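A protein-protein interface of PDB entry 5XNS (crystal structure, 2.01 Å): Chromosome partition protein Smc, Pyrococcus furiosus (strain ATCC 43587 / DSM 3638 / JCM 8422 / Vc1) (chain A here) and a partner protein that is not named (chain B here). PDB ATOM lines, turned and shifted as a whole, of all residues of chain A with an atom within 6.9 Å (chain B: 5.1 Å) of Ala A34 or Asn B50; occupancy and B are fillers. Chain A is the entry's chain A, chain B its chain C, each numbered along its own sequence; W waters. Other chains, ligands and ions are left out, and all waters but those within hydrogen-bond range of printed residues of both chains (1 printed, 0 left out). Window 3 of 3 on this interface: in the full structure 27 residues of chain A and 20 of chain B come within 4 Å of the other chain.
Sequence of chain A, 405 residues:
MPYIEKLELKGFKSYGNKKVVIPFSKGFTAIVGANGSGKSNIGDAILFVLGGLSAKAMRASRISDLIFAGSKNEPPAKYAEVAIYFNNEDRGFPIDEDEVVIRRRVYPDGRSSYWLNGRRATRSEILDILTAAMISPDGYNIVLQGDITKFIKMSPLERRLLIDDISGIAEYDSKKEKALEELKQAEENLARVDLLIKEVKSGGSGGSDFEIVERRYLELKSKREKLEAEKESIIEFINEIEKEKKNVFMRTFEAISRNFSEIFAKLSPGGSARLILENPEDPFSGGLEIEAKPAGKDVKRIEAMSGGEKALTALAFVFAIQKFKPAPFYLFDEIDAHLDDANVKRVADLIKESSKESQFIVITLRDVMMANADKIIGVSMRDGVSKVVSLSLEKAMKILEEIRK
Among the printed residues, pairs that only touch across the chains: Ala A34 with Phe B47 (3.6 Å), Ser A37 with Asn B50 (3.6 Å), Ser A380 with Asn B50 (3.7 Å), Ala A34 with Asn B50 (3.7 Å), Val A32 with Leu B46 (3.8 Å) and Gly A33 with Phe B47 (3.8 Å).
The backbone carbonyl oxygen (O) of Ala A34 is in hydrogen-bond range of the side-chain hydroxyl (OG) of Ser A37 (2.7 Å).
The side-chain amino group (NZ) of Lys A39 sits at hydrogen-bond distance from the backbone carbonyl oxygen (O) of Gly A33 (3.3 Å).
O of Val A32 sits at hydrogen-bond distance from N of Val A379 (2.8 Å).
The backbone carbonyl oxygen (O) of Ala A34 lies within hydrogen-bond range of the side-chain amino group (NZ) of Lys A39 (3.5 Å).
OG of Ser A37 lies within hydrogen-bond range of N of Lys A39 (3.2 Å).
O of Ser A37 sits at hydrogen-bond distance from OG of Ser A386.
The side-chain amide oxygen (OD1) of Asn B50 lies within hydrogen-bond range of the backbone NH (N) of Met A381 (2.7 Å).
OG of Ser A380 lies within hydrogen-bond range of OE1 of Glu B49 (2.7 Å).
Of the printed residues of chain B, Gly A33 touches Phe B47 (3.8 Å).
Printed residues of chain B within 4 Å of Ala A34: Phe B47 (3.6 Å) and Asn B50 (3.7 Å).
Of the printed residues of chain A, Leu B46 touches Val A32 (3.8 Å).
Printed residues of chain A within 4 Å of Phe B47: Gly A33 (3.8 Å) and Ala A34 (3.6 Å).
Leu B48 touches none of the printed residues of chain A.
Of the 17 printed residues of chain A, 6 touch a printed residue of chain B.
Along chain A the printed residues that touch a printed residue of chain B span positions 32 to 381.
Of the 8 printed residues of chain B, 4 touch a printed residue of chain A.
Hydrophobic or aromatic side chains of chain B that line the printed part of chain A: Leu B46 and Phe B47.
Among the printed residues, no Asp or Glu carboxylate lies within 4 Å of a Lys or Arg side-chain nitrogen of the other chain.
Water W1 lies within hydrogen-bond range of the backbone carbonyl oxygen (O) of Val A379 (2.7 Å), the backbone carbonyl oxygen (O) of Leu B46 (2.8 Å) and the backbone NH (N) of Ala A34 (2.9 Å).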
ATOM      1  N   VAL A  32      19.220   8.901  -9.473  1.00  0.00           N
ATOM      2  CA  VAL A  32      18.481   7.685  -9.152  1.00  0.00           C
ATOM      3  C   VAL A  32      19.035   6.509  -9.940  1.00  0.00           C
ATOM      4  O   VAL A  32      19.762   6.671 -10.921  1.00  0.00           O
ATOM      5  CB  VAL A  32      16.970   7.837  -9.409  1.00  0.00           C
ATOM      6  CG1 VAL A  32      16.480   9.172  -8.833  1.00  0.00           C
ATOM      7  CG2 VAL A  32      16.683   7.743 -10.910  1.00  0.00           C
ATOM      8  N   GLY A  33      18.657   5.320  -9.496  1.00  0.00           N
ATOM      9  CA  GLY A  33      19.111   4.076 -10.086  1.00  0.00           C
ATOM     10  C   GLY A  33      19.162   2.985  -9.039  1.00  0.00           C
ATOM     11  O   GLY A  33      18.961   3.216  -7.844  1.00  0.00           O
ATOM     12  N   ALA A  34      19.424   1.769  -9.516  1.00  0.00           N
ATOM     13  CA  ALA A  34      19.575   0.617  -8.636  1.00  0.00           C
ATOM     14  C   ALA A  34      20.699   0.835  -7.626  1.00  0.00           C
ATOM     15  O   ALA A  34      21.654   1.584  -7.870  1.00  0.00           O
ATOM     16  CB  ALA A  34      19.885  -0.643  -9.463  1.00  0.00           C
ATOM     17  N   ASN A  35      20.597   0.151  -6.490  1.00  0.00           N
ATOM     18  CA  ASN A  35      21.750   0.051  -5.615  1.00  0.00           C
ATOM     19  C   ASN A  35      22.836  -0.734  -6.337  1.00  0.00           C
ATOM     20  O   ASN A  35      22.571  -1.765  -6.954  1.00  0.00           O
ATOM     21  CB  ASN A  35      21.371  -0.601  -4.280  1.00  0.00           C
ATOM     22  CG  ASN A  35      20.636   0.381  -3.320  1.00  0.00           C
ATOM     23  OD1 ASN A  35      20.720   1.626  -3.457  1.00  0.00           O
ATOM     24  ND2 ASN A  35      19.909  -0.181  -2.358  1.00  0.00           N
ATOM     25  N   GLY A  36      24.049  -0.210  -6.321  1.00  0.00           N
ATOM     26  CA  GLY A  36      25.111  -0.782  -7.117  1.00  0.00           C
ATOM     27  C   GLY A  36      25.246  -0.183  -8.498  1.00  0.00           C
ATOM     28  O   GLY A  36      26.117  -0.617  -9.263  1.00  0.00           O
ATOM     29  N   SER A  37      24.432   0.811  -8.844  1.00  0.00           N
ATOM     30  CA  SER A  37      24.552   1.402 -10.172  1.00  0.00           C
ATOM     31  C   SER A  37      25.751   2.326 -10.291  1.00  0.00           C
ATOM     32  O   SER A  37      26.177   2.616 -11.412  1.00  0.00           O
ATOM     33  CB  SER A  37      23.298   2.201 -10.523  1.00  0.00           C
ATOM     34  OG  SER A  37      23.060   3.171  -9.519  1.00  0.00           O
ATOM     35  N   GLY A  38      26.291   2.807  -9.175  1.00  0.00           N
ATOM     36  CA  GLY A  38      27.237   3.906  -9.197  1.00  0.00           C
ATOM     37  C   GLY A  38      26.625   5.270  -8.946  1.00  0.00           C
ATOM     38  O   GLY A  38      27.350   6.275  -9.008  1.00  0.00           O
ATOM     39  N   LYS A  39      25.313   5.347  -8.675  1.00  0.00           N
ATOM     40  CA  LYS A  39      24.709   6.639  -8.357  1.00  0.00           C
ATOM     41  C   LYS A  39      25.337   7.259  -7.108  1.00  0.00           C
ATOM     42  O   LYS A  39      25.495   8.482  -7.029  1.00  0.00           O
ATOM     43  CB  LYS A  39      23.196   6.507  -8.181  1.00  0.00           C
ATOM     44  CG  LYS A  39      22.722   5.694  -6.973  1.00  0.00           C
ATOM     45  CD  LYS A  39      21.191   5.642  -6.947  1.00  0.00           C
ATOM     46  CE  LYS A  39      20.627   5.208  -5.596  1.00  0.00           C
ATOM     47  NZ  LYS A  39      20.935   3.801  -5.276  1.00  0.00           N
ATOM     48  N   SER A  40      25.704   6.444  -6.121  1.00  0.00           N
ATOM     49  CA  SER A  40      26.268   7.033  -4.906  1.00  0.00           C
ATOM     50  C   SER A  40      27.704   7.510  -5.096  1.00  0.00           C
ATOM     51  O   SER A  40      28.157   8.403  -4.354  1.00  0.00           O
ATOM     52  CB  SER A  40      26.172   6.038  -3.749  1.00  0.00           C
ATOM     53  OG  SER A  40      24.792   5.814  -3.445  1.00  0.00           O
ATOM     54  N   THR A 364      18.894   8.903  -4.619  1.00  0.00           N
ATOM     55  CA  THR A 364      17.764   8.177  -4.045  1.00  0.00           C
ATOM     56  C   THR A 364      17.258   7.162  -5.053  1.00  0.00           C
ATOM     57  O   THR A 364      17.523   7.276  -6.252  1.00  0.00           O
ATOM     58  CB  THR A 364      16.636   9.137  -3.626  1.00  0.00           C
ATOM     59  OG1 THR A 364      15.609   8.426  -2.915  1.00  0.00           O
ATOM     60  CG2 THR A 364      16.015   9.810  -4.841  1.00  0.00           C
ATOM     61  N   LEU A 365      16.556   6.143  -4.544  1.00  0.00           N
ATOM     62  CA  LEU A 365      15.687   5.306  -5.369  1.00  0.00           C
ATOM     63  C   LEU A 365      14.258   5.296  -4.841  1.00  0.00           C
ATOM     64  O   LEU A 365      13.493   4.378  -5.155  1.00  0.00           O
ATOM     65  CB  LEU A 365      16.214   3.870  -5.490  1.00  0.00           C
ATOM     66  CG  LEU A 365      16.789   3.164  -4.256  1.00  0.00           C
ATOM     67  CD1 LEU A 365      15.743   3.014  -3.144  1.00  0.00           C
ATOM     68  CD2 LEU A 365      17.393   1.804  -4.622  1.00  0.00           C
ATOM     69  N   VAL A 379      21.068   6.506 -13.363  1.00  0.00           N
ATOM     70  CA  VAL A 379      22.384   5.887 -13.433  1.00  0.00           C
ATOM     71  C   VAL A 379      22.184   4.387 -13.502  1.00  0.00           C
ATOM     72  O   VAL A 379      21.390   3.824 -12.736  1.00  0.00           O
ATOM     73  CB  VAL A 379      23.265   6.250 -12.222  1.00  0.00           C
ATOM     74  CG1 VAL A 379      24.699   5.704 -12.408  1.00  0.00           C
ATOM     75  CG2 VAL A 379      23.274   7.746 -11.994  1.00  0.00           C
ATOM     76  N   SER A 380      22.907   3.743 -14.411  1.00  0.00           N
ATOM     77  CA  SER A 380      22.892   2.293 -14.508  1.00  0.00           C
ATOM     78  C   SER A 380      24.281   1.813 -14.892  1.00  0.00           C
ATOM     79  O   SER A 380      25.030   2.514 -15.575  1.00  0.00           O
ATOM     80  CB  SER A 380      21.859   1.815 -15.537  1.00  0.00           C
ATOM     81  OG  SER A 380      22.230   2.285 -16.817  1.00  0.00           O
ATOM     82  N   MET A 381      24.621   0.612 -14.441  1.00  0.00           N
ATOM     83  CA  MET A 381      25.936   0.041 -14.678  1.00  0.00           C
ATOM     84  C   MET A 381      25.834  -0.958 -15.821  1.00  0.00           C
ATOM     85  O   MET A 381      25.098  -1.947 -15.724  1.00  0.00           O
ATOM     86  CB  MET A 381      26.493  -0.626 -13.424  1.00  0.00           C
ATOM     87  CG  MET A 381      27.997  -0.695 -13.448  1.00  0.00           C
ATOM     88  SD  MET A 381      28.716  -1.306 -11.919  1.00  0.00           S
ATOM     89  CE  MET A 381      28.224  -3.028 -11.998  1.00  0.00           C
ATOM     90  N   ARG A 382      26.553  -0.676 -16.912  1.00  0.00           N
ATOM     91  CA  ARG A 382      26.584  -1.506 -18.116  1.00  0.00           C
ATOM     92  C   ARG A 382      28.003  -2.059 -18.266  1.00  0.00           C
ATOM     93  O   ARG A 382      28.924  -1.326 -18.646  1.00  0.00           O
ATOM     94  CB  ARG A 382      26.159  -0.681 -19.332  1.00  0.00           C
ATOM     95  CG  ARG A 382      26.063  -1.450 -20.647  1.00  0.00           C
ATOM     96  CD  ARG A 382      25.304  -0.644 -21.708  1.00  0.00           C
ATOM     97  NE  ARG A 382      26.162   0.357 -22.345  1.00  0.00           N
ATOM     98  CZ  ARG A 382      26.851   0.154 -23.472  1.00  0.00           C
ATOM     99  NH1 ARG A 382      26.790  -1.018 -24.098  1.00  0.00           N
ATOM    100  NH2 ARG A 382      27.615   1.131 -23.976  1.00  0.00           N
ATOM    101  N   VAL A 385      30.579  -0.599 -15.927  1.00  0.00           N
ATOM    102  CA  VAL A 385      30.810   0.816 -16.179  1.00  0.00           C
ATOM    103  C   VAL A 385      29.490   1.563 -15.990  1.00  0.00           C
ATOM    104  O   VAL A 385      28.455   1.156 -16.532  1.00  0.00           O
ATOM    105  CB  VAL A 385      31.383   1.048 -17.589  1.00  0.00           C
ATOM    106  CG1 VAL A 385      31.711   2.512 -17.794  1.00  0.00           C
ATOM    107  CG2 VAL A 385      32.643   0.189 -17.807  1.00  0.00           C
ATOM    108  N   SER A 386      29.523   2.644 -15.217  1.00  0.00           N
ATOM    109  CA  SER A 386      28.314   3.417 -14.962  1.00  0.00           C
ATOM    110  C   SER A 386      28.056   4.397 -16.096  1.00  0.00           C
ATOM    111  O   SER A 386      28.980   5.038 -16.601  1.00  0.00           O
ATOM    112  CB  SER A 386      28.427   4.182 -13.637  1.00  0.00           C
ATOM    113  OG  SER A 386      28.507   3.291 -12.536  1.00  0.00           O
ATOM    114  N   LEU B  45      12.798   1.209 -15.420  1.00  0.00           N
ATOM    115  CA  LEU B  45      13.665   0.972 -16.564  1.00  0.00           C
ATOM    116  C   LEU B  45      15.136   0.966 -16.145  1.00  0.00           C
ATOM    117  O   LEU B  45      15.909   0.104 -16.585  1.00  0.00           O
ATOM    118  CB  LEU B  45      13.393   2.014 -17.644  1.00  0.00           C
ATOM    119  CG  LEU B  45      12.026   1.859 -18.315  1.00  0.00           C
ATOM    120  CD1 LEU B  45      11.700   3.102 -19.121  1.00  0.00           C
ATOM    121  CD2 LEU B  45      11.949   0.585 -19.189  1.00  0.00           C
ATOM    122  N   LEU B  46      15.534   1.874 -15.251  1.00  0.00           N
ATOM    123  CA  LEU B  46      16.930   1.860 -14.815  1.00  0.00           C
ATOM    124  C   LEU B  46      17.249   0.593 -14.037  1.00  0.00           C
ATOM    125  O   LEU B  46      18.366   0.067 -14.141  1.00  0.00           O
ATOM    126  CB  LEU B  46      17.249   3.104 -13.990  1.00  0.00           C
ATOM    127  CG  LEU B  46      17.115   4.357 -14.844  1.00  0.00           C
ATOM    128  CD1 LEU B  46      16.790   5.563 -13.963  1.00  0.00           C
ATOM    129  CD2 LEU B  46      18.363   4.585 -15.674  1.00  0.00           C
ATOM    130  N   PHE B  47      16.291   0.098 -13.238  1.00  0.00           N
ATOM    131  CA  PHE B  47      16.450  -1.214 -12.609  1.00  0.00           C
ATOM    132  C   PHE B  47      16.669  -2.298 -13.664  1.00  0.00           C
ATOM    133  O   PHE B  47      17.586  -3.123 -13.556  1.00  0.00           O
ATOM    134  CB  PHE B  47      15.225  -1.550 -11.750  1.00  0.00           C
ATOM    135  CG  PHE B  47      15.115  -0.745 -10.464  1.00  0.00           C
ATOM    136  CD1 PHE B  47      16.119   0.126 -10.066  1.00  0.00           C
ATOM    137  CD2 PHE B  47      13.992  -0.867  -9.657  1.00  0.00           C
ATOM    138  CE1 PHE B  47      16.013   0.851  -8.881  1.00  0.00           C
ATOM    139  CE2 PHE B  47      13.874  -0.146  -8.477  1.00  0.00           C
ATOM    140  CZ  PHE B  47      14.885   0.710  -8.088  1.00  0.00           C
ATOM    141  N   LEU B  48      15.828  -2.305 -14.702  1.00  0.00           N
ATOM    142  CA  LEU B  48      15.961  -3.317 -15.740  1.00  0.00           C
ATOM    143  C   LEU B  48      17.284  -3.168 -16.479  1.00  0.00           C
ATOM    144  O   LEU B  48      17.895  -4.163 -16.882  1.00  0.00           O
ATOM    145  CB  LEU B  48      14.772  -3.245 -16.703  1.00  0.00           C
ATOM    146  CG  LEU B  48      13.455  -3.846 -16.165  1.00  0.00           C
ATOM    147  CD1 LEU B  48      12.285  -3.423 -17.018  1.00  0.00           C
ATOM    148  CD2 LEU B  48      13.508  -5.369 -16.069  1.00  0.00           C
ATOM    149  N   GLU B  49      17.752  -1.937 -16.660  1.00  0.00           N
ATOM    150  CA  GLU B  49      19.000  -1.768 -17.388  1.00  0.00           C
ATOM    151  C   GLU B  49      20.192  -2.209 -16.551  1.00  0.00           C
ATOM    152  O   GLU B  49      21.136  -2.794 -17.087  1.00  0.00           O
ATOM    153  CB  GLU B  49      19.171  -0.326 -17.844  1.00  0.00           C
ATOM    154  CG  GLU B  49      20.423  -0.149 -18.684  1.00  0.00           C
ATOM    155  CD  GLU B  49      20.507   1.202 -19.327  1.00  0.00           C
ATOM    156  OE1 GLU B  49      20.266   2.201 -18.612  1.00  0.00           O
ATOM    157  OE2 GLU B  49      20.810   1.254 -20.547  1.00  0.00           O
ATOM    158  N   ASN B  50      20.152  -1.972 -15.238  1.00  0.00           N
ATOM    159  CA  ASN B  50      21.256  -2.399 -14.390  1.00  0.00           C
ATOM    160  C   ASN B  50      21.363  -3.918 -14.334  1.00  0.00           C
ATOM    161  O   ASN B  50      22.447  -4.449 -14.084  1.00  0.00           O
ATOM    162  CB  ASN B  50      21.090  -1.819 -12.986  1.00  0.00           C
ATOM    163  CG  ASN B  50      22.409  -1.705 -12.253  1.00  0.00           C
ATOM    164  OD1 ASN B  50      23.273  -0.900 -12.626  1.00  0.00           O
ATOM    165  ND2 ASN B  50      22.584  -2.521 -11.225  1.00  0.00           N
ATOM    166  N   MET B  51      20.257  -4.626 -14.556  1.00  0.00           N
ATOM    167  CA  MET B  51      20.252  -6.082 -14.627  1.00  0.00           C
ATOM    168  C   MET B  51      20.512  -6.611 -16.031  1.00  0.00           C
ATOM    169  O   MET B  51      20.474  -7.829 -16.230  1.00  0.00           O
ATOM    170  CB  MET B  51      18.916  -6.649 -14.137  1.00  0.00           C
ATOM    171  CG  MET B  51      18.541  -6.282 -12.731  1.00  0.00           C
ATOM    172  SD  MET B  51      16.867  -6.870 -12.352  1.00  0.00           S
ATOM    173  CE  MET B  51      15.838  -5.777 -13.297  1.00  0.00           C
ATOM    174  N   GLY B  52      20.755  -5.737 -17.003  1.00  0.00           N
ATOM    175  CA  GLY B  52      21.039  -6.177 -18.351  1.00  0.00           C
ATOM    176  C   GLY B  52      19.844  -6.647 -19.151  1.00  0.00           C
ATOM    177  O   GLY B  52      20.031  -7.271 -20.197  1.00  0.00           O
HETATM  178  O   HOH W   1      20.021   1.489 -12.320  1.00  0.00           O
